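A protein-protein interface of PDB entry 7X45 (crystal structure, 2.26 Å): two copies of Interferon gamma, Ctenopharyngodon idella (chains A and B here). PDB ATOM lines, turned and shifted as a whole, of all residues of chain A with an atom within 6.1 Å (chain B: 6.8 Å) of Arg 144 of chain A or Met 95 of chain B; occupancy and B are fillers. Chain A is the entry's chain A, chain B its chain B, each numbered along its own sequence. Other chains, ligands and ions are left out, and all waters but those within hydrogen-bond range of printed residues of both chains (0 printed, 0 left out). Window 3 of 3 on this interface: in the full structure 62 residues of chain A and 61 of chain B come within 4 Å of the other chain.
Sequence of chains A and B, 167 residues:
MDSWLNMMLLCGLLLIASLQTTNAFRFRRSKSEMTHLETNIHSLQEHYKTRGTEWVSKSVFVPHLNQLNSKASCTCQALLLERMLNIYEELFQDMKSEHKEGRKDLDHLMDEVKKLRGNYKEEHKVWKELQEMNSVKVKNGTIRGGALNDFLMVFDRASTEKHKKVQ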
ATOM      1  N   LEU A  44       7.632  19.438 -21.632  1.00  0.00           N
ATOM      2  CA  LEU A  44       8.230  20.565 -20.872  1.00  0.00           C
ATOM      3  C   LEU A  44       7.967  20.358 -19.371  1.00  0.00           C
ATOM      4  O   LEU A  44       8.895  20.600 -18.581  1.00  0.00           O
ATOM      5  CB  LEU A  44       7.650  21.878 -21.411  1.00  0.00           C
ATOM      6  CG  LEU A  44       8.455  23.147 -21.133  1.00  0.00           C
ATOM      7  CD1 LEU A  44       9.892  22.997 -21.620  1.00  0.00           C
ATOM      8  CD2 LEU A  44       7.787  24.370 -21.757  1.00  0.00           C
ATOM      9  N   TYR A  48      10.397  19.801 -16.057  1.00  0.00           N
ATOM     10  CA  TYR A  48      10.214  20.742 -14.914  1.00  0.00           C
ATOM     11  C   TYR A  48       9.252  20.126 -13.881  1.00  0.00           C
ATOM     12  O   TYR A  48       8.297  20.806 -13.459  1.00  0.00           O
ATOM     13  CB  TYR A  48       9.736  22.119 -15.410  1.00  0.00           C
ATOM     14  CG  TYR A  48      10.784  22.999 -16.058  1.00  0.00           C
ATOM     15  CD1 TYR A  48      11.074  22.888 -17.409  1.00  0.00           C
ATOM     16  CD2 TYR A  48      11.474  23.966 -15.336  1.00  0.00           C
ATOM     17  CE1 TYR A  48      12.033  23.685 -18.019  1.00  0.00           C
ATOM     18  CE2 TYR A  48      12.447  24.760 -15.928  1.00  0.00           C
ATOM     19  CZ  TYR A  48      12.726  24.626 -17.278  1.00  0.00           C
ATOM     20  OH  TYR A  48      13.669  25.418 -17.877  1.00  0.00           O
ATOM     21  N   LYS A 137       6.172  36.862 -10.453  1.00  0.00           N
ATOM     22  CA  LYS A 137       7.605  36.450 -10.430  1.00  0.00           C
ATOM     23  C   LYS A 137       7.801  35.268 -11.392  1.00  0.00           C
ATOM     24  O   LYS A 137       7.567  34.094 -11.004  1.00  0.00           O
ATOM     25  CB  LYS A 137       8.078  36.063  -9.018  1.00  0.00           C
ATOM     26  CG  LYS A 137       7.531  36.865  -7.838  1.00  0.00           C
ATOM     27  CD  LYS A 137       7.512  38.377  -8.014  1.00  0.00           C
ATOM     28  CE  LYS A 137       6.781  39.094  -6.894  1.00  0.00           C
ATOM     29  NZ  LYS A 137       5.856  40.137  -7.402  1.00  0.00           N
ATOM     30  N   VAL A 138       8.234  35.591 -12.609  1.00  0.00           N
ATOM     31  CA  VAL A 138       8.489  34.648 -13.735  1.00  0.00           C
ATOM     32  C   VAL A 138       9.564  33.606 -13.341  1.00  0.00           C
ATOM     33  O   VAL A 138       9.535  32.485 -13.908  1.00  0.00           O
ATOM     34  CB  VAL A 138       8.867  35.478 -14.983  1.00  0.00           C
ATOM     35  CG1 VAL A 138      10.175  36.250 -14.816  1.00  0.00           C
ATOM     36  CG2 VAL A 138       8.902  34.628 -16.232  1.00  0.00           C
ATOM     37  N   LYS A 139      10.451  33.926 -12.386  1.00  0.00           N
ATOM     38  CA  LYS A 139      11.639  33.094 -12.018  1.00  0.00           C
ATOM     39  C   LYS A 139      11.336  32.219 -10.792  1.00  0.00           C
ATOM     40  O   LYS A 139      12.292  31.724 -10.172  1.00  0.00           O
ATOM     41  CB  LYS A 139      12.855  33.995 -11.767  1.00  0.00           C
ATOM     42  CG  LYS A 139      12.997  35.159 -12.740  1.00  0.00           C
ATOM     43  CD  LYS A 139      14.391  35.734 -12.844  1.00  0.00           C
ATOM     44  CE  LYS A 139      14.450  36.953 -13.741  1.00  0.00           C
ATOM     45  NZ  LYS A 139      15.850  37.302 -14.083  1.00  0.00           N
ATOM     46  N   ASN A 140      10.053  32.025 -10.470  1.00  0.00           N
ATOM     47  CA  ASN A 140       9.575  31.251  -9.296  1.00  0.00           C
ATOM     48  C   ASN A 140       9.042  29.895  -9.769  1.00  0.00           C
ATOM     49  O   ASN A 140       8.332  29.872 -10.792  1.00  0.00           O
ATOM     50  CB  ASN A 140       8.480  32.008  -8.540  1.00  0.00           C
ATOM     51  CG  ASN A 140       8.132  31.354  -7.220  1.00  0.00           C
ATOM     52  OD1 ASN A 140       8.906  31.427  -6.269  1.00  0.00           O
ATOM     53  ND2 ASN A 140       6.982  30.712  -7.139  1.00  0.00           N
ATOM     54  N   GLY A 141       9.346  28.822  -9.030  1.00  0.00           N
ATOM     55  CA  GLY A 141       8.951  27.438  -9.370  1.00  0.00           C
ATOM     56  C   GLY A 141       7.442  27.276  -9.432  1.00  0.00           C
ATOM     57  O   GLY A 141       6.935  26.782 -10.462  1.00  0.00           O
ATOM     58  N   THR A 142       6.740  27.680  -8.371  1.00  0.00           N
ATOM     59  CA  THR A 142       5.260  27.572  -8.246  1.00  0.00           C
ATOM     60  C   THR A 142       4.600  28.312  -9.411  1.00  0.00           C
ATOM     61  O   THR A 142       3.637  27.751  -9.995  1.00  0.00           O
ATOM     62  CB  THR A 142       4.760  28.083  -6.887  1.00  0.00           C
ATOM     63  OG1 THR A 142       4.993  27.042  -5.939  1.00  0.00           O
ATOM     64  CG2 THR A 142       3.296  28.472  -6.895  1.00  0.00           C
ATOM     65  N   ILE A 143       5.085  29.515  -9.737  1.00  0.00           N
ATOM     66  CA  ILE A 143       4.536  30.327 -10.860  1.00  0.00           C
ATOM     67  C   ILE A 143       4.876  29.617 -12.169  1.00  0.00           C
ATOM     68  O   ILE A 143       3.975  29.486 -12.997  1.00  0.00           O
ATOM     69  CB  ILE A 143       5.031  31.782 -10.803  1.00  0.00           C
ATOM     70  CG1 ILE A 143       4.501  32.454  -9.534  1.00  0.00           C
ATOM     71  CG2 ILE A 143       4.673  32.552 -12.075  1.00  0.00           C
ATOM     72  CD1 ILE A 143       4.421  33.958  -9.603  1.00  0.00           C
ATOM     73  N   ARG A 144       6.111  29.150 -12.338  1.00  0.00           N
ATOM     74  CA  ARG A 144       6.498  28.314 -13.506  1.00  0.00           C
ATOM     75  C   ARG A 144       5.466  27.189 -13.678  1.00  0.00           C
ATOM     76  O   ARG A 144       4.906  27.072 -14.768  1.00  0.00           O
ATOM     77  CB  ARG A 144       7.895  27.713 -13.329  1.00  0.00           C
ATOM     78  CG  ARG A 144       8.950  28.296 -14.253  1.00  0.00           C
ATOM     79  CD  ARG A 144      10.168  27.398 -14.408  1.00  0.00           C
ATOM     80  NE  ARG A 144      11.282  27.682 -13.503  1.00  0.00           N
ATOM     81  CZ  ARG A 144      12.051  28.781 -13.540  1.00  0.00           C
ATOM     82  NH1 ARG A 144      11.834  29.739 -14.432  1.00  0.00           N
ATOM     83  NH2 ARG A 144      13.036  28.920 -12.664  1.00  0.00           N
ATOM     84  N   GLY A 145       5.247  26.392 -12.630  1.00  0.00           N
ATOM     85  CA  GLY A 145       4.369  25.204 -12.661  1.00  0.00           C
ATOM     86  C   GLY A 145       2.939  25.596 -12.969  1.00  0.00           C
ATOM     87  O   GLY A 145       2.389  25.119 -13.989  1.00  0.00           O
ATOM     88  N   GLY A 146       2.387  26.496 -12.150  1.00  0.00           N
ATOM     89  CA  GLY A 146       1.062  27.103 -12.369  1.00  0.00           C
ATOM     90  C   GLY A 146       0.908  27.632 -13.780  1.00  0.00           C
ATOM     91  O   GLY A 146      -0.170  27.460 -14.376  1.00  0.00           O
ATOM     92  N   ALA A 147       1.940  28.291 -14.307  1.00  0.00           N
ATOM     93  CA  ALA A 147       1.922  28.924 -15.647  1.00  0.00           C
ATOM     94  C   ALA A 147       1.875  27.847 -16.737  1.00  0.00           C
ATOM     95  O   ALA A 147       1.095  28.012 -17.699  1.00  0.00           O
ATOM     96  CB  ALA A 147       3.128  29.830 -15.821  1.00  0.00           C
ATOM     97  N   LEU A 148       2.697  26.804 -16.626  1.00  0.00           N
ATOM     98  CA  LEU A 148       2.682  25.653 -17.576  1.00  0.00           C
ATOM     99  C   LEU A 148       1.314  24.960 -17.566  1.00  0.00           C
ATOM    100  O   LEU A 148       0.772  24.690 -18.671  1.00  0.00           O
ATOM    101  CB  LEU A 148       3.806  24.677 -17.209  1.00  0.00           C
ATOM    102  CG  LEU A 148       5.216  25.217 -17.448  1.00  0.00           C
ATOM    103  CD1 LEU A 148       6.276  24.267 -16.912  1.00  0.00           C
ATOM    104  CD2 LEU A 148       5.436  25.507 -18.929  1.00  0.00           C
ATOM    105  N   ASN A 149       0.753  24.706 -16.376  1.00  0.00           N
ATOM    106  CA  ASN A 149      -0.615  24.124 -16.218  1.00  0.00           C
ATOM    107  C   ASN A 149      -1.632  24.987 -16.985  1.00  0.00           C
ATOM    108  O   ASN A 149      -2.509  24.415 -17.672  1.00  0.00           O
ATOM    109  CB  ASN A 149      -0.990  23.974 -14.740  1.00  0.00           C
ATOM    110  CG  ASN A 149      -2.347  23.326 -14.534  1.00  0.00           C
ATOM    111  OD1 ASN A 149      -2.641  22.294 -15.136  1.00  0.00           O
ATOM    112  ND2 ASN A 149      -3.187  23.920 -13.703  1.00  0.00           N
ATOM    113  N   TYR B  88       4.019  35.114 -20.831  1.00  0.00           N
ATOM    114  CA  TYR B  88       4.458  33.773 -21.292  1.00  0.00           C
ATOM    115  C   TYR B  88       5.728  33.922 -22.137  1.00  0.00           C
ATOM    116  O   TYR B  88       6.632  33.090 -22.030  1.00  0.00           O
ATOM    117  CB  TYR B  88       3.323  33.054 -22.017  1.00  0.00           C
ATOM    118  CG  TYR B  88       2.444  32.241 -21.102  1.00  0.00           C
ATOM    119  CD1 TYR B  88       2.945  31.189 -20.351  1.00  0.00           C
ATOM    120  CD2 TYR B  88       1.103  32.541 -20.972  1.00  0.00           C
ATOM    121  CE1 TYR B  88       2.122  30.450 -19.513  1.00  0.00           C
ATOM    122  CE2 TYR B  88       0.267  31.802 -20.151  1.00  0.00           C
ATOM    123  CZ  TYR B  88       0.775  30.757 -19.412  1.00  0.00           C
ATOM    124  OH  TYR B  88      -0.063  30.066 -18.579  1.00  0.00           O
ATOM    125  N   GLU B  90       8.116  36.283 -21.818  1.00  0.00           N
ATOM    126  CA  GLU B  90       9.207  36.560 -20.837  1.00  0.00           C
ATOM    127  C   GLU B  90       9.547  35.259 -20.107  1.00  0.00           C
ATOM    128  O   GLU B  90      10.750  34.945 -19.997  1.00  0.00           O
ATOM    129  CB  GLU B  90       8.809  37.582 -19.763  1.00  0.00           C
ATOM    130  CG  GLU B  90       8.151  38.867 -20.251  1.00  0.00           C
ATOM    131  CD  GLU B  90       7.135  39.462 -19.267  1.00  0.00           C
ATOM    132  OE1 GLU B  90       6.194  40.185 -19.718  1.00  0.00           O
ATOM    133  OE2 GLU B  90       7.285  39.219 -18.043  1.00  0.00           O
ATOM    134  N   LEU B  91       8.520  34.536 -19.634  1.00  0.00           N
ATOM    135  CA  LEU B  91       8.677  33.234 -18.919  1.00  0.00           C
ATOM    136  C   LEU B  91       9.466  32.245 -19.773  1.00  0.00           C
ATOM    137  O   LEU B  91      10.425  31.634 -19.260  1.00  0.00           O
ATOM    138  CB  LEU B  91       7.312  32.625 -18.589  1.00  0.00           C
ATOM    139  CG  LEU B  91       7.395  31.180 -18.087  1.00  0.00           C
ATOM    140  CD1 LEU B  91       7.875  31.132 -16.640  1.00  0.00           C
ATOM    141  CD2 LEU B  91       6.066  30.458 -18.231  1.00  0.00           C
ATOM    142  N   PHE B  92       9.014  32.017 -21.002  1.00  0.00           N
ATOM    143  CA  PHE B  92       9.628  31.014 -21.899  1.00  0.00           C
ATOM    144  C   PHE B  92      11.084  31.446 -22.112  1.00  0.00           C
ATOM    145  O   PHE B  92      11.978  30.589 -22.115  1.00  0.00           O
ATOM    146  CB  PHE B  92       8.769  30.811 -23.154  1.00  0.00           C
ATOM    147  CG  PHE B  92       7.432  30.125 -22.942  1.00  0.00           C
ATOM    148  CD1 PHE B  92       7.222  29.236 -21.898  1.00  0.00           C
ATOM    149  CD2 PHE B  92       6.379  30.348 -23.819  1.00  0.00           C
ATOM    150  CE1 PHE B  92       5.996  28.603 -21.730  1.00  0.00           C
ATOM    151  CE2 PHE B  92       5.149  29.732 -23.641  1.00  0.00           C
ATOM    152  CZ  PHE B  92       4.958  28.860 -22.596  1.00  0.00           C
ATOM    153  N   GLN B  93      11.337  32.750 -22.185  1.00  0.00           N
ATOM    154  CA  GLN B  93      12.711  33.289 -22.392  1.00  0.00           C
ATOM    155  C   GLN B  93      13.548  33.013 -21.136  1.00  0.00           C
ATOM    156  O   GLN B  93      14.651  32.494 -21.263  1.00  0.00           O
ATOM    157  CB  GLN B  93      12.654  34.779 -22.730  1.00  0.00           C
ATOM    158  CG  GLN B  93      14.027  35.410 -22.871  1.00  0.00           C
ATOM    159  CD  GLN B  93      14.768  34.770 -24.014  1.00  0.00           C
ATOM    160  OE1 GLN B  93      14.558  35.135 -25.168  1.00  0.00           O
ATOM    161  NE2 GLN B  93      15.617  33.802 -23.711  1.00  0.00           N
ATOM    162  N   ASP B  94      13.027  33.364 -19.962  1.00  0.00           N
ATOM    163  CA  ASP B  94      13.745  33.202 -18.676  1.00  0.00           C
ATOM    164  C   ASP B  94      14.105  31.721 -18.515  1.00  0.00           C
ATOM    165  O   ASP B  94      15.265  31.443 -18.130  1.00  0.00           O
ATOM    166  CB  ASP B  94      12.920  33.796 -17.532  1.00  0.00           C
ATOM    167  CG  ASP B  94      13.534  33.562 -16.166  1.00  0.00           C
ATOM    168  OD1 ASP B  94      14.231  34.476 -15.682  1.00  0.00           O
ATOM    169  OD2 ASP B  94      13.306  32.469 -15.599  1.00  0.00           O
ATOM    170  N   MET B  95      13.177  30.805 -18.842  1.00  0.00           N
ATOM    171  CA  MET B  95      13.394  29.329 -18.767  1.00  0.00           C
ATOM    172  C   MET B  95      14.546  28.926 -19.694  1.00  0.00           C
ATOM    173  O   MET B  95      15.348  28.055 -19.290  1.00  0.00           O
ATOM    174  CB  MET B  95      12.148  28.538 -19.188  1.00  0.00           C
ATOM    175  CG  MET B  95      10.997  28.614 -18.212  1.00  0.00           C
ATOM    176  SD  MET B  95       9.522  27.732 -18.807  1.00  0.00           S
ATOM    177  CE  MET B  95       9.569  26.277 -17.763  1.00  0.00           C
ATOM    178  N   LYS B  96      14.597  29.517 -20.895  1.00  0.00           N
ATOM    179  CA  LYS B  96      15.570  29.182 -21.975  1.00  0.00           C
ATOM    180  C   LYS B  96      17.004  29.408 -21.488  1.00  0.00           C
ATOM    181  O   LYS B  96      17.803  28.464 -21.550  1.00  0.00           O
ATOM    182  CB  LYS B  96      15.302  30.024 -23.228  1.00  0.00           C
ATOM    183  CG  LYS B  96      14.644  29.254 -24.368  1.00  0.00           C
ATOM    184  CD  LYS B  96      13.846  30.116 -25.339  1.00  0.00           C
ATOM    185  CE  LYS B  96      14.406  30.164 -26.745  1.00  0.00           C
ATOM    186  NZ  LYS B  96      13.323  30.229 -27.758  1.00  0.00           N
ATOM    187  N   SER B  97      17.315  30.620 -21.029  1.00  0.00           N
ATOM    188  CA  SER B  97      18.663  31.000 -20.525  1.00  0.00           C
ATOM    189  C   SER B  97      19.086  30.090 -19.362  1.00  0.00           C
ATOM    190  O   SER B  97      20.290  29.830 -19.241  1.00  0.00           O
ATOM    191  CB  SER B  97      18.702  32.453 -20.137  1.00  0.00           C
ATOM    192  OG  SER B  97      17.490  32.845 -19.533  1.00  0.00           O
ATOM    193  N   GLU B  98      18.140  29.617 -18.542  1.00  0.00           N
ATOM    194  CA  GLU B  98      18.431  28.726 -17.387  1.00  0.00           C
ATOM    195  C   GLU B  98      18.270  27.266 -17.831  1.00  0.00           C
ATOM    196  O   GLU B  98      19.261  26.730 -18.346  1.00  0.00           O
ATOM    197  CB  GLU B  98      17.537  29.097 -16.198  1.00  0.00           C
ATOM    198  CG  GLU B  98      16.200  28.382 -16.153  1.00  0.00           C
ATOM    199  CD  GLU B  98      15.169  29.052 -15.258  1.00  0.00           C
ATOM    200  OE1 GLU B  98      15.504  29.370 -14.095  1.00  0.00           O
ATOM    201  OE2 GLU B  98      14.041  29.275 -15.736  1.00  0.00           O
ATOM    202  N   LEU B 106      10.184  24.600 -25.689  1.00  0.00           N
ATOM    203  CA  LEU B 106      10.220  26.028 -25.289  1.00  0.00           C
ATOM    204  C   LEU B 106      10.228  26.885 -26.553  1.00  0.00           C
ATOM    205  O   LEU B 106       9.566  27.927 -26.550  1.00  0.00           O
ATOM    206  CB  LEU B 106      11.484  26.244 -24.448  1.00  0.00           C
ATOM    207  CG  LEU B 106      11.403  27.261 -23.313  1.00  0.00           C
ATOM    208  CD1 LEU B 106      10.073  27.175 -22.574  1.00  0.00           C
ATOM    209  CD2 LEU B 106      12.559  27.057 -22.344  1.00  0.00           C
ATOM    210  N   MET B 110       7.304  29.512 -27.687  1.00  0.00           N
ATOM    211  CA  MET B 110       7.605  30.955 -27.826  1.00  0.00           C
ATOM    212  C   MET B 110       7.240  31.402 -29.242  1.00  0.00           C
ATOM    213  O   MET B 110       6.677  32.491 -29.378  1.00  0.00           O
ATOM    214  CB  MET B 110       9.064  31.304 -27.540  1.00  0.00           C
ATOM    215  CG  MET B 110       9.154  32.720 -26.992  1.00  0.00           C
ATOM    216  SD  MET B 110      10.795  33.206 -26.460  1.00  0.00           S
ATOM    217  CE  MET B 110      10.944  32.331 -24.908  1.00  0.00           C
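Among the printed residues, pairs that only touch across the chains: Leu 44 of chain A with Leu 106 of chain B, Val 138 of chain A with Glu 90 of chain B, Val 138 of chain A with Leu 91 of chain B, Arg 144 of chain A with Leu 91 of chain B, Arg 144 of chain A with Met 95 of chain B, Ala 147 of chain A with Leu 91 of chain B and Leu 148 of chain A with Met 95 of chain B.
Along chain B the printed residues that touch a printed residue of chain A span positions 88 to 106.
Printed residues of chain A that touch a printed residue of chain B: Leu 44, Tyr 48, Val 138, Lys 139, Arg 144, Ala 147 and Leu 148.
Among the printed residues, 12 pairs touch across the chains.
Among the printed residues, Asp or Glu carboxylates within 4 Å of a Lys or Arg side-chain nitrogen of the other chain: Lys 139 of chain A with Asp 94 of chain B, Arg 144 of chain A with Asp 94 of chain B and Arg 144 of chain A with Glu 98 of chain B.
O of Asp 94 of chain B is in hydrogen-bond range of OG of Ser 97 of chain B, 3.0 Å away.
Of chain A, only Tyr 48 (3.4 Å), Arg 144 (3.6 Å) and Leu 148 (3.95 Å) come within 4 Å of Met 95 of chain B.
Printed residues of chain A within 4 Å of Tyr 88 of chain B: Ala 147 (2.5 Å).
Printed residues of chain B within 4 Å of Lys 139 of chain A: Asp 94.
Printed residues of chain B within 4 Å of Ala 147 of chain A: Tyr 88 and Leu 91.
Lys 96 of chain B touches none of the printed residues of chain A.
Gly 141 of chain A touches none of the printed residues of chain B.
The nearest residue of chain A that does not touch Met 95 of chain B is Leu 44 of chain A (4.7 Å).
The side-chain carboxylate (OE2) of Glu 98 of chain B is in salt-bridge range of the guanidinium group (NH1) of Arg 144 of chain A (2.6 Å).
The side-chain hydroxyl (OH) of Tyr 48 of chain A sits at hydrogen-bond distance from the backbone carbonyl oxygen (O) of Met 95 of chain B.
OD1 of Asp 94 of chain B lies within salt-bridge range of NZ of Lys 139 of chain A.
The backbone carbonyl oxygen (O) of Ala 147 of chain A sits at hydrogen-bond distance from the side-chain hydroxyl (OH) of Tyr 88 of chain B, at 2.5 Å.
The guanidinium group (NH1) of Arg 144 of chain A is in salt-bridge range of the side-chain carboxylate (OD2) of Asp 94 of chain B (3.3 Å).
No position is printed for both chains.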
